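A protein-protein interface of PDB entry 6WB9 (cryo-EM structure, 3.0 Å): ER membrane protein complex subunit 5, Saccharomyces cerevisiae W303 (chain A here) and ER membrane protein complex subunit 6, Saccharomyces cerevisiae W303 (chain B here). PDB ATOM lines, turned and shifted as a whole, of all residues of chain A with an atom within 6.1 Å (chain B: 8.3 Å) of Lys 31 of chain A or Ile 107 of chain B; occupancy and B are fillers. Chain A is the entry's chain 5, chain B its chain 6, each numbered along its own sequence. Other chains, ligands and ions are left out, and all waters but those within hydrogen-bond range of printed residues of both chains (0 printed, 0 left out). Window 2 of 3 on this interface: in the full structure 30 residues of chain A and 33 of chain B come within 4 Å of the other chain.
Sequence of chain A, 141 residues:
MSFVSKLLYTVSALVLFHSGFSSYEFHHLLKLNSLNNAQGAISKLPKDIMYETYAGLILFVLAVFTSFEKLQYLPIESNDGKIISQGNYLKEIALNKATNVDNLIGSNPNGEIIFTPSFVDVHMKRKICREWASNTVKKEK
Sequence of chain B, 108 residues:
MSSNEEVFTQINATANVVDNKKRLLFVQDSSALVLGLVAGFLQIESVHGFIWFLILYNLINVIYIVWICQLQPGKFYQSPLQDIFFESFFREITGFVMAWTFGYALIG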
ATOM      1  N   GLY A  20     -31.615 -17.113  17.054  1.00  0.00           N
ATOM      2  CA  GLY A  20     -31.147 -18.330  16.418  1.00  0.00           C
ATOM      3  C   GLY A  20     -32.090 -18.816  15.339  1.00  0.00           C
ATOM      4  O   GLY A  20     -31.650 -19.307  14.301  1.00  0.00           O
ATOM      5  N   PHE A  21     -33.399 -18.654  15.550  1.00  0.00           N
ATOM      6  CA  PHE A  21     -34.362 -18.999  14.510  1.00  0.00           C
ATOM      7  C   PHE A  21     -34.262 -18.047  13.324  1.00  0.00           C
ATOM      8  O   PHE A  21     -34.373 -18.474  12.170  1.00  0.00           O
ATOM      9  CB  PHE A  21     -35.775 -18.991  15.086  1.00  0.00           C
ATOM     10  CG  PHE A  21     -36.843 -19.258  14.070  1.00  0.00           C
ATOM     11  CD1 PHE A  21     -37.003 -20.524  13.535  1.00  0.00           C
ATOM     12  CD2 PHE A  21     -37.694 -18.245  13.659  1.00  0.00           C
ATOM     13  CE1 PHE A  21     -37.987 -20.774  12.601  1.00  0.00           C
ATOM     14  CE2 PHE A  21     -38.680 -18.488  12.727  1.00  0.00           C
ATOM     15  CZ  PHE A  21     -38.827 -19.754  12.197  1.00  0.00           C
ATOM     16  N   SER A  23     -31.481 -16.411  12.428  1.00  0.00           N
ATOM     17  CA  SER A  23     -30.235 -16.741  11.748  1.00  0.00           C
ATOM     18  C   SER A  23     -30.339 -18.057  10.990  1.00  0.00           C
ATOM     19  O   SER A  23     -29.711 -18.210   9.939  1.00  0.00           O
ATOM     20  CB  SER A  23     -29.090 -16.798  12.756  1.00  0.00           C
ATOM     21  OG  SER A  23     -27.865 -17.099  12.115  1.00  0.00           O
ATOM     22  N   TYR A  24     -31.136 -19.004  11.495  1.00  0.00           N
ATOM     23  CA  TYR A  24     -31.413 -20.232  10.759  1.00  0.00           C
ATOM     24  C   TYR A  24     -32.179 -19.946   9.478  1.00  0.00           C
ATOM     25  O   TYR A  24     -31.853 -20.500   8.422  1.00  0.00           O
ATOM     26  CB  TYR A  24     -32.201 -21.203  11.638  1.00  0.00           C
ATOM     27  CG  TYR A  24     -32.914 -22.290  10.869  1.00  0.00           C
ATOM     28  CD1 TYR A  24     -32.204 -23.320  10.269  1.00  0.00           C
ATOM     29  CD2 TYR A  24     -34.299 -22.292  10.751  1.00  0.00           C
ATOM     30  CE1 TYR A  24     -32.848 -24.314   9.565  1.00  0.00           C
ATOM     31  CE2 TYR A  24     -34.954 -23.284  10.048  1.00  0.00           C
ATOM     32  CZ  TYR A  24     -34.222 -24.293   9.458  1.00  0.00           C
ATOM     33  OH  TYR A  24     -34.865 -25.288   8.758  1.00  0.00           O
ATOM     34  N   PHE A  26     -32.193 -17.081   7.839  1.00  0.00           N
ATOM     35  CA  PHE A  26     -31.323 -16.350   6.926  1.00  0.00           C
ATOM     36  C   PHE A  26     -30.291 -17.263   6.276  1.00  0.00           C
ATOM     37  O   PHE A  26     -30.039 -17.158   5.071  1.00  0.00           O
ATOM     38  CB  PHE A  26     -30.629 -15.205   7.656  1.00  0.00           C
ATOM     39  CG  PHE A  26     -29.768 -14.369   6.764  1.00  0.00           C
ATOM     40  CD1 PHE A  26     -30.340 -13.429   5.925  1.00  0.00           C
ATOM     41  CD2 PHE A  26     -28.391 -14.528   6.754  1.00  0.00           C
ATOM     42  CE1 PHE A  26     -29.558 -12.663   5.094  1.00  0.00           C
ATOM     43  CE2 PHE A  26     -27.606 -13.768   5.922  1.00  0.00           C
ATOM     44  CZ  PHE A  26     -28.192 -12.834   5.093  1.00  0.00           C
ATOM     45  N   HIS A  27     -29.684 -18.166   7.044  1.00  0.00           N
ATOM     46  CA  HIS A  27     -28.647 -19.013   6.478  1.00  0.00           C
ATOM     47  C   HIS A  27     -29.205 -20.186   5.688  1.00  0.00           C
ATOM     48  O   HIS A  27     -28.463 -20.794   4.914  1.00  0.00           O
ATOM     49  CB  HIS A  27     -27.716 -19.515   7.580  1.00  0.00           C
ATOM     50  CG  HIS A  27     -26.748 -18.481   8.058  1.00  0.00           C
ATOM     51  ND1 HIS A  27     -27.067 -17.553   9.024  1.00  0.00           N
ATOM     52  CD2 HIS A  27     -25.475 -18.212   7.684  1.00  0.00           C
ATOM     53  CE1 HIS A  27     -26.028 -16.766   9.235  1.00  0.00           C
ATOM     54  NE2 HIS A  27     -25.050 -17.144   8.433  1.00  0.00           N
ATOM     55  N   HIS A  28     -30.484 -20.517   5.850  1.00  0.00           N
ATOM     56  CA  HIS A  28     -31.115 -21.505   4.992  1.00  0.00           C
ATOM     57  C   HIS A  28     -31.903 -20.875   3.854  1.00  0.00           C
ATOM     58  O   HIS A  28     -32.406 -21.600   2.992  1.00  0.00           O
ATOM     59  CB  HIS A  28     -32.009 -22.427   5.820  1.00  0.00           C
ATOM     60  CG  HIS A  28     -31.244 -23.463   6.581  1.00  0.00           C
ATOM     61  ND1 HIS A  28     -30.283 -23.142   7.516  1.00  0.00           N
ATOM     62  CD2 HIS A  28     -31.274 -24.816   6.525  1.00  0.00           C
ATOM     63  CE1 HIS A  28     -29.766 -24.252   8.011  1.00  0.00           C
ATOM     64  NE2 HIS A  28     -30.351 -25.281   7.429  1.00  0.00           N
ATOM     65  N   LEU A  29     -32.024 -19.549   3.834  1.00  0.00           N
ATOM     66  CA  LEU A  29     -32.409 -18.846   2.621  1.00  0.00           C
ATOM     67  C   LEU A  29     -31.202 -18.456   1.783  1.00  0.00           C
ATOM     68  O   LEU A  29     -31.334 -18.283   0.568  1.00  0.00           O
ATOM     69  CB  LEU A  29     -33.224 -17.596   2.962  1.00  0.00           C
ATOM     70  CG  LEU A  29     -34.742 -17.684   2.789  1.00  0.00           C
ATOM     71  CD1 LEU A  29     -35.092 -17.966   1.339  1.00  0.00           C
ATOM     72  CD2 LEU A  29     -35.347 -18.740   3.699  1.00  0.00           C
ATOM     73  N   LEU A  30     -30.030 -18.310   2.405  1.00  0.00           N
ATOM     74  CA  LEU A  30     -28.813 -18.062   1.639  1.00  0.00           C
ATOM     75  C   LEU A  30     -28.346 -19.308   0.905  1.00  0.00           C
ATOM     76  O   LEU A  30     -27.734 -19.201  -0.163  1.00  0.00           O
ATOM     77  CB  LEU A  30     -27.696 -17.563   2.553  1.00  0.00           C
ATOM     78  CG  LEU A  30     -27.422 -16.063   2.628  1.00  0.00           C
ATOM     79  CD1 LEU A  30     -26.083 -15.827   3.306  1.00  0.00           C
ATOM     80  CD2 LEU A  30     -27.448 -15.426   1.250  1.00  0.00           C
ATOM     81  N   LYS A  31     -28.600 -20.491   1.467  1.00  0.00           N
ATOM     82  CA  LYS A  31     -28.205 -21.726   0.801  1.00  0.00           C
ATOM     83  C   LYS A  31     -29.086 -22.013  -0.406  1.00  0.00           C
ATOM     84  O   LYS A  31     -28.624 -22.629  -1.372  1.00  0.00           O
ATOM     85  CB  LYS A  31     -28.245 -22.893   1.784  1.00  0.00           C
ATOM     86  CG  LYS A  31     -27.096 -22.900   2.776  1.00  0.00           C
ATOM     87  CD  LYS A  31     -27.360 -23.851   3.930  1.00  0.00           C
ATOM     88  CE  LYS A  31     -26.315 -23.684   5.022  1.00  0.00           C
ATOM     89  NZ  LYS A  31     -26.614 -24.517   6.217  1.00  0.00           N
ATOM     90  N   LEU A  32     -30.346 -21.579  -0.373  1.00  0.00           N
ATOM     91  CA  LEU A  32     -31.209 -21.703  -1.540  1.00  0.00           C
ATOM     92  C   LEU A  32     -30.922 -20.642  -2.593  1.00  0.00           C
ATOM     93  O   LEU A  32     -31.258 -20.846  -3.764  1.00  0.00           O
ATOM     94  CB  LEU A  32     -32.680 -21.628  -1.125  1.00  0.00           C
ATOM     95  CG  LEU A  32     -33.200 -22.740  -0.211  1.00  0.00           C
ATOM     96  CD1 LEU A  32     -34.692 -22.584   0.022  1.00  0.00           C
ATOM     97  CD2 LEU A  32     -32.889 -24.110  -0.787  1.00  0.00           C
ATOM     98  N   ASN A  33     -30.315 -19.523  -2.209  1.00  0.00           N
ATOM     99  CA  ASN A  33     -29.983 -18.457  -3.143  1.00  0.00           C
ATOM    100  C   ASN A  33     -28.560 -18.560  -3.675  1.00  0.00           C
ATOM    101  O   ASN A  33     -28.110 -17.654  -4.382  1.00  0.00           O
ATOM    102  CB  ASN A  33     -30.197 -17.092  -2.485  1.00  0.00           C
ATOM    103  CG  ASN A  33     -31.653 -16.815  -2.178  1.00  0.00           C
ATOM    104  OD1 ASN A  33     -32.550 -17.335  -2.840  1.00  0.00           O
ATOM    105  ND2 ASN A  33     -31.899 -15.992  -1.165  1.00  0.00           N
ATOM    106  N   SER A  34     -27.844 -19.636  -3.350  1.00  0.00           N
ATOM    107  CA  SER A  34     -26.518 -19.888  -3.898  1.00  0.00           C
ATOM    108  C   SER A  34     -26.529 -21.034  -4.903  1.00  0.00           C
ATOM    109  O   SER A  34     -25.479 -21.614  -5.193  1.00  0.00           O
ATOM    110  CB  SER A  34     -25.520 -20.174  -2.777  1.00  0.00           C
ATOM    111  OG  SER A  34     -25.848 -21.372  -2.096  1.00  0.00           O
ATOM    112  N   LEU A  35     -27.701 -21.370  -5.432  1.00  0.00           N
ATOM    113  CA  LEU A  35     -27.848 -22.483  -6.360  1.00  0.00           C
ATOM    114  C   LEU A  35     -28.342 -21.997  -7.718  1.00  0.00           C
ATOM    115  O   LEU A  35     -29.282 -21.206  -7.798  1.00  0.00           O
ATOM    116  CB  LEU A  35     -28.809 -23.524  -5.790  1.00  0.00           C
ATOM    117  CG  LEU A  35     -28.481 -24.012  -4.378  1.00  0.00           C
ATOM    118  CD1 LEU A  35     -29.627 -24.826  -3.798  1.00  0.00           C
ATOM    119  CD2 LEU A  35     -27.188 -24.814  -4.366  1.00  0.00           C
ATOM    120  N   LEU B  37     -22.928 -21.331  21.597  1.00  0.00           N
ATOM    121  CA  LEU B  37     -24.206 -21.186  20.902  1.00  0.00           C
ATOM    122  C   LEU B  37     -24.270 -19.894  20.096  1.00  0.00           C
ATOM    123  O   LEU B  37     -24.808 -19.878  18.986  1.00  0.00           O
ATOM    124  CB  LEU B  37     -25.362 -21.231  21.898  1.00  0.00           C
ATOM    125  CG  LEU B  37     -26.045 -22.567  22.168  1.00  0.00           C
ATOM    126  CD1 LEU B  37     -27.335 -22.310  22.906  1.00  0.00           C
ATOM    127  CD2 LEU B  37     -26.303 -23.321  20.883  1.00  0.00           C
ATOM    128  N   VAL B  38     -23.723 -18.804  20.632  1.00  0.00           N
ATOM    129  CA  VAL B  38     -23.748 -17.535  19.910  1.00  0.00           C
ATOM    130  C   VAL B  38     -22.726 -17.531  18.771  1.00  0.00           C
ATOM    131  O   VAL B  38     -23.003 -17.002  17.689  1.00  0.00           O
ATOM    132  CB  VAL B  38     -23.545 -16.373  20.902  1.00  0.00           C
ATOM    133  CG1 VAL B  38     -23.387 -15.039  20.196  1.00  0.00           C
ATOM    134  CG2 VAL B  38     -24.731 -16.291  21.840  1.00  0.00           C
ATOM    135  N   ALA B  39     -21.561 -18.164  18.957  1.00  0.00           N
ATOM    136  CA  ALA B  39     -20.612 -18.313  17.860  1.00  0.00           C
ATOM    137  C   ALA B  39     -21.119 -19.252  16.775  1.00  0.00           C
ATOM    138  O   ALA B  39     -20.658 -19.164  15.635  1.00  0.00           O
ATOM    139  CB  ALA B  39     -19.271 -18.820  18.384  1.00  0.00           C
ATOM    140  N   GLY B  40     -22.042 -20.156  17.104  1.00  0.00           N
ATOM    141  CA  GLY B  40     -22.691 -20.940  16.071  1.00  0.00           C
ATOM    142  C   GLY B  40     -23.849 -20.228  15.410  1.00  0.00           C
ATOM    143  O   GLY B  40     -24.114 -20.450  14.226  1.00  0.00           O
ATOM    144  N   PHE B  41     -24.560 -19.378  16.157  1.00  0.00           N
ATOM    145  CA  PHE B  41     -25.666 -18.616  15.582  1.00  0.00           C
ATOM    146  C   PHE B  41     -25.163 -17.558  14.614  1.00  0.00           C
ATOM    147  O   PHE B  41     -25.834 -17.254  13.623  1.00  0.00           O
ATOM    148  CB  PHE B  41     -26.493 -17.936  16.678  1.00  0.00           C
ATOM    149  CG  PHE B  41     -27.371 -18.868  17.475  1.00  0.00           C
ATOM    150  CD1 PHE B  41     -27.485 -20.213  17.158  1.00  0.00           C
ATOM    151  CD2 PHE B  41     -28.098 -18.378  18.548  1.00  0.00           C
ATOM    152  CE1 PHE B  41     -28.291 -21.047  17.902  1.00  0.00           C
ATOM    153  CE2 PHE B  41     -28.907 -19.205  19.292  1.00  0.00           C
ATOM    154  CZ  PHE B  41     -29.004 -20.539  18.968  1.00  0.00           C
ATOM    155  N   LEU B  42     -23.995 -16.985  14.890  1.00  0.00           N
ATOM    156  CA  LEU B  42     -23.395 -15.984  14.025  1.00  0.00           C
ATOM    157  C   LEU B  42     -22.587 -16.589  12.889  1.00  0.00           C
ATOM    158  O   LEU B  42     -22.134 -15.836  12.020  1.00  0.00           O
ATOM    159  CB  LEU B  42     -22.500 -15.061  14.846  1.00  0.00           C
ATOM    160  CG  LEU B  42     -23.222 -14.193  15.867  1.00  0.00           C
ATOM    161  CD1 LEU B  42     -22.216 -13.556  16.789  1.00  0.00           C
ATOM    162  CD2 LEU B  42     -24.025 -13.145  15.144  1.00  0.00           C
ATOM    163  N   GLN B  43     -22.406 -17.915  12.896  1.00  0.00           N
ATOM    164  CA  GLN B  43     -21.653 -18.673  11.893  1.00  0.00           C
ATOM    165  C   GLN B  43     -20.218 -18.159  11.772  1.00  0.00           C
ATOM    166  O   GLN B  43     -19.772 -17.705  10.718  1.00  0.00           O
ATOM    167  CB  GLN B  43     -22.371 -18.666  10.540  1.00  0.00           C
ATOM    168  CG  GLN B  43     -23.689 -19.409  10.550  1.00  0.00           C
ATOM    169  CD  GLN B  43     -23.520 -20.885  10.293  1.00  0.00           C
ATOM    170  OE1 GLN B  43     -22.932 -21.288   9.292  1.00  0.00           O
ATOM    171  NE2 GLN B  43     -24.034 -21.703  11.196  1.00  0.00           N
ATOM    172  N   TRP B 100     -20.215 -24.780  19.878  1.00  0.00           N
ATOM    173  CA  TRP B 100     -19.922 -24.086  18.632  1.00  0.00           C
ATOM    174  C   TRP B 100     -20.281 -24.946  17.435  1.00  0.00           C
ATOM    175  O   TRP B 100     -20.924 -24.474  16.496  1.00  0.00           O
ATOM    176  CB  TRP B 100     -18.440 -23.731  18.610  1.00  0.00           C
ATOM    177  CG  TRP B 100     -17.997 -22.823  17.533  1.00  0.00           C
ATOM    178  CD1 TRP B 100     -18.766 -21.998  16.776  1.00  0.00           C
ATOM    179  CD2 TRP B 100     -16.652 -22.634  17.098  1.00  0.00           C
ATOM    180  NE1 TRP B 100     -17.980 -21.304  15.891  1.00  0.00           N
ATOM    181  CE2 TRP B 100     -16.676 -21.680  16.071  1.00  0.00           C
ATOM    182  CE3 TRP B 100     -15.427 -23.187  17.476  1.00  0.00           C
ATOM    183  CZ2 TRP B 100     -15.526 -21.262  15.422  1.00  0.00           C
ATOM    184  CZ3 TRP B 100     -14.288 -22.771  16.831  1.00  0.00           C
ATOM    185  CH2 TRP B 100     -14.343 -21.820  15.814  1.00  0.00           C
ATOM    186  N   THR B 101     -19.867 -26.214  17.458  1.00  0.00           N
ATOM    187  CA  THR B 101     -20.237 -27.147  16.404  1.00  0.00           C
ATOM    188  C   THR B 101     -21.734 -27.414  16.390  1.00  0.00           C
ATOM    189  O   THR B 101     -22.320 -27.523  15.310  1.00  0.00           O
ATOM    190  CB  THR B 101     -19.470 -28.453  16.571  1.00  0.00           C
ATOM    191  OG1 THR B 101     -19.507 -28.844  17.944  1.00  0.00           O
ATOM    192  CG2 THR B 101     -18.032 -28.278  16.172  1.00  0.00           C
ATOM    193  N   PHE B 102     -22.370 -27.467  17.568  1.00  0.00           N
ATOM    194  CA  PHE B 102     -23.816 -27.668  17.634  1.00  0.00           C
ATOM    195  C   PHE B 102     -24.574 -26.497  17.019  1.00  0.00           C
ATOM    196  O   PHE B 102     -25.468 -26.693  16.190  1.00  0.00           O
ATOM    197  CB  PHE B 102     -24.244 -27.882  19.085  1.00  0.00           C
ATOM    198  CG  PHE B 102     -25.689 -28.247  19.245  1.00  0.00           C
ATOM    199  CD1 PHE B 102     -26.107 -29.551  19.052  1.00  0.00           C
ATOM    200  CD2 PHE B 102     -26.629 -27.290  19.598  1.00  0.00           C
ATOM    201  CE1 PHE B 102     -27.432 -29.894  19.201  1.00  0.00           C
ATOM    202  CE2 PHE B 102     -27.955 -27.626  19.744  1.00  0.00           C
ATOM    203  CZ  PHE B 102     -28.357 -28.931  19.546  1.00  0.00           C
ATOM    204  N   GLY B 103     -24.220 -25.269  17.404  1.00  0.00           N
ATOM    205  CA  GLY B 103     -24.895 -24.108  16.855  1.00  0.00           C
ATOM    206  C   GLY B 103     -24.556 -23.842  15.405  1.00  0.00           C
ATOM    207  O   GLY B 103     -25.402 -23.366  14.649  1.00  0.00           O
ATOM    208  N   TYR B 104     -23.326 -24.148  14.994  1.00  0.00           N
ATOM    209  CA  TYR B 104     -22.919 -23.934  13.612  1.00  0.00           C
ATOM    210  C   TYR B 104     -23.569 -24.950  12.689  1.00  0.00           C
ATOM    211  O   TYR B 104     -23.896 -24.635  11.541  1.00  0.00           O
ATOM    212  CB  TYR B 104     -21.398 -24.011  13.522  1.00  0.00           C
ATOM    213  CG  TYR B 104     -20.804 -23.549  12.217  1.00  0.00           C
ATOM    214  CD1 TYR B 104     -20.534 -22.207  11.995  1.00  0.00           C
ATOM    215  CD2 TYR B 104     -20.488 -24.458  11.215  1.00  0.00           C
ATOM    216  CE1 TYR B 104     -19.983 -21.781  10.808  1.00  0.00           C
ATOM    217  CE2 TYR B 104     -19.938 -24.039  10.023  1.00  0.00           C
ATOM    218  CZ  TYR B 104     -19.687 -22.699   9.827  1.00  0.00           C
ATOM    219  OH  TYR B 104     -19.137 -22.275   8.642  1.00  0.00           O
ATOM    220  N   ALA B 105     -23.766 -26.177  13.174  1.00  0.00           N
ATOM    221  CA  ALA B 105     -24.461 -27.179  12.387  1.00  0.00           C
ATOM    222  C   ALA B 105     -25.963 -26.948  12.378  1.00  0.00           C
ATOM    223  O   ALA B 105     -26.627 -27.245  11.381  1.00  0.00           O
ATOM    224  CB  ALA B 105     -24.143 -28.559  12.934  1.00  0.00           C
ATOM    225  N   LEU B 106     -26.515 -26.423  13.469  1.00  0.00           N
ATOM    226  CA  LEU B 106     -27.952 -26.206  13.555  1.00  0.00           C
ATOM    227  C   LEU B 106     -28.416 -24.957  12.821  1.00  0.00           C
ATOM    228  O   LEU B 106     -29.624 -24.785  12.638  1.00  0.00           O
ATOM    229  CB  LEU B 106     -28.378 -26.124  15.021  1.00  0.00           C
ATOM    230  CG  LEU B 106     -29.682 -26.832  15.373  1.00  0.00           C
ATOM    231  CD1 LEU B 106     -29.555 -28.321  15.115  1.00  0.00           C
ATOM    232  CD2 LEU B 106     -30.048 -26.570  16.818  1.00  0.00           C
ATOM    233  N   ILE B 107     -27.504 -24.086  12.405  1.00  0.00           N
ATOM    234  CA  ILE B 107     -27.881 -22.885  11.670  1.00  0.00           C
ATOM    235  C   ILE B 107     -27.472 -23.018  10.210  1.00  0.00           C
ATOM    236  O   ILE B 107     -26.373 -23.478   9.901  1.00  0.00           O
ATOM    237  CB  ILE B 107     -27.260 -21.618  12.297  1.00  0.00           C
ATOM    238  CG1 ILE B 107     -27.787 -21.379  13.716  1.00  0.00           C
ATOM    239  CG2 ILE B 107     -27.503 -20.408  11.418  1.00  0.00           C
ATOM    240  CD1 ILE B 107     -29.264 -21.533  13.879  1.00  0.00           C
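Among the printed residues, merely in contact across the chains: Gly 20 of chain A with Phe 41 of chain B, Gly 20 of chain A with Ile 107 of chain B, Ser 23 of chain A with Ile 107 of chain B, Tyr 24 of chain A with Leu 106 of chain B, Tyr 24 of chain A with Ile 107 of chain B, His 27 of chain A with Gln 43 of chain B, His 27 of chain A with Ile 107 of chain B, His 28 of chain A with Ile 107 of chain B and Lys 31 of chain A with Ile 107 of chain B.
Of the printed residues of chain B, Gly 20 of chain A touches Phe 41 and Ile 107.
Of the printed residues of chain B, His 27 of chain A touches Gln 43 (3.4 Å) and Ile 107 (3.8 Å).
Of the printed residues of chain B, His 28 of chain A touches Ile 107 (3.4 Å).
Leu 29 of chain A touches none of the printed residues of chain B.
Lys 31 of chain A touches just one residue of chain B: Ile 107.
Printed residues of chain A within 4 Å of Ile 107 of chain B: Gly 20 (3.3 Å), Ser 23 (3.4 Å), Tyr 24 (3.7 Å), His 27 (3.8 Å), His 28 (3.4 Å) and Lys 31 (3.8 Å).
The nearest residue of chain B that does not touch Lys 31 of chain A is Gln 43 of chain B (5.8 Å).
The nearest printed residue of chain A that does not touch Phe 41 of chain B is His 27 of chain A (4.4 Å).
Printed residues of chain B that touch a printed residue of chain A: Phe 41, Gln 43, Leu 106 and Ile 107.
Along chain B the printed residues that touch a printed residue of chain A span positions 41 to 107.
Printed residues of chain A that touch a printed residue of chain B: Gly 20, Ser 23, Tyr 24, His 27, His 28 and Lys 31.
Hydrophobic or aromatic side chains of chain A within 4 Å of the printed part of chain B: Tyr 24, His 27 and His 28.
ND1 of His 27 of chain A sits at hydrogen-bond distance from O of Ser 23 of chain A, at 2.9 Å.
A ring nitrogen (ND1) of His 28 of chain A lies within hydrogen-bond range of the backbone carbonyl oxygen of Tyr 24 of chain A.
The backbone carbonyl oxygen (O) of Lys 31 of chain A lies within hydrogen-bond range of the side-chain hydroxyl (OG) of Ser 34 of chain A (3.1 Å).
O of Gly 40 of chain B sits at hydrogen-bond distance from NE2 of Gln 43 of chain B (3.3 Å).
The side-chain amide nitrogen (NE2) of Gln 43 of chain B sits at hydrogen-bond distance from the backbone carbonyl oxygen (O) of Tyr 104 of chain B, at 3.0 Å.
NE2 of Gln 43 of chain B lies within hydrogen-bond range of O of Ile 107 of chain B, at 3.2 Å.
The backbone carbonyl oxygen (O) of Phe 41 of chain B is in hydrogen-bond range of the side-chain hydroxyl (OG) of Ser 23 of chain A, 2.5 Å away.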
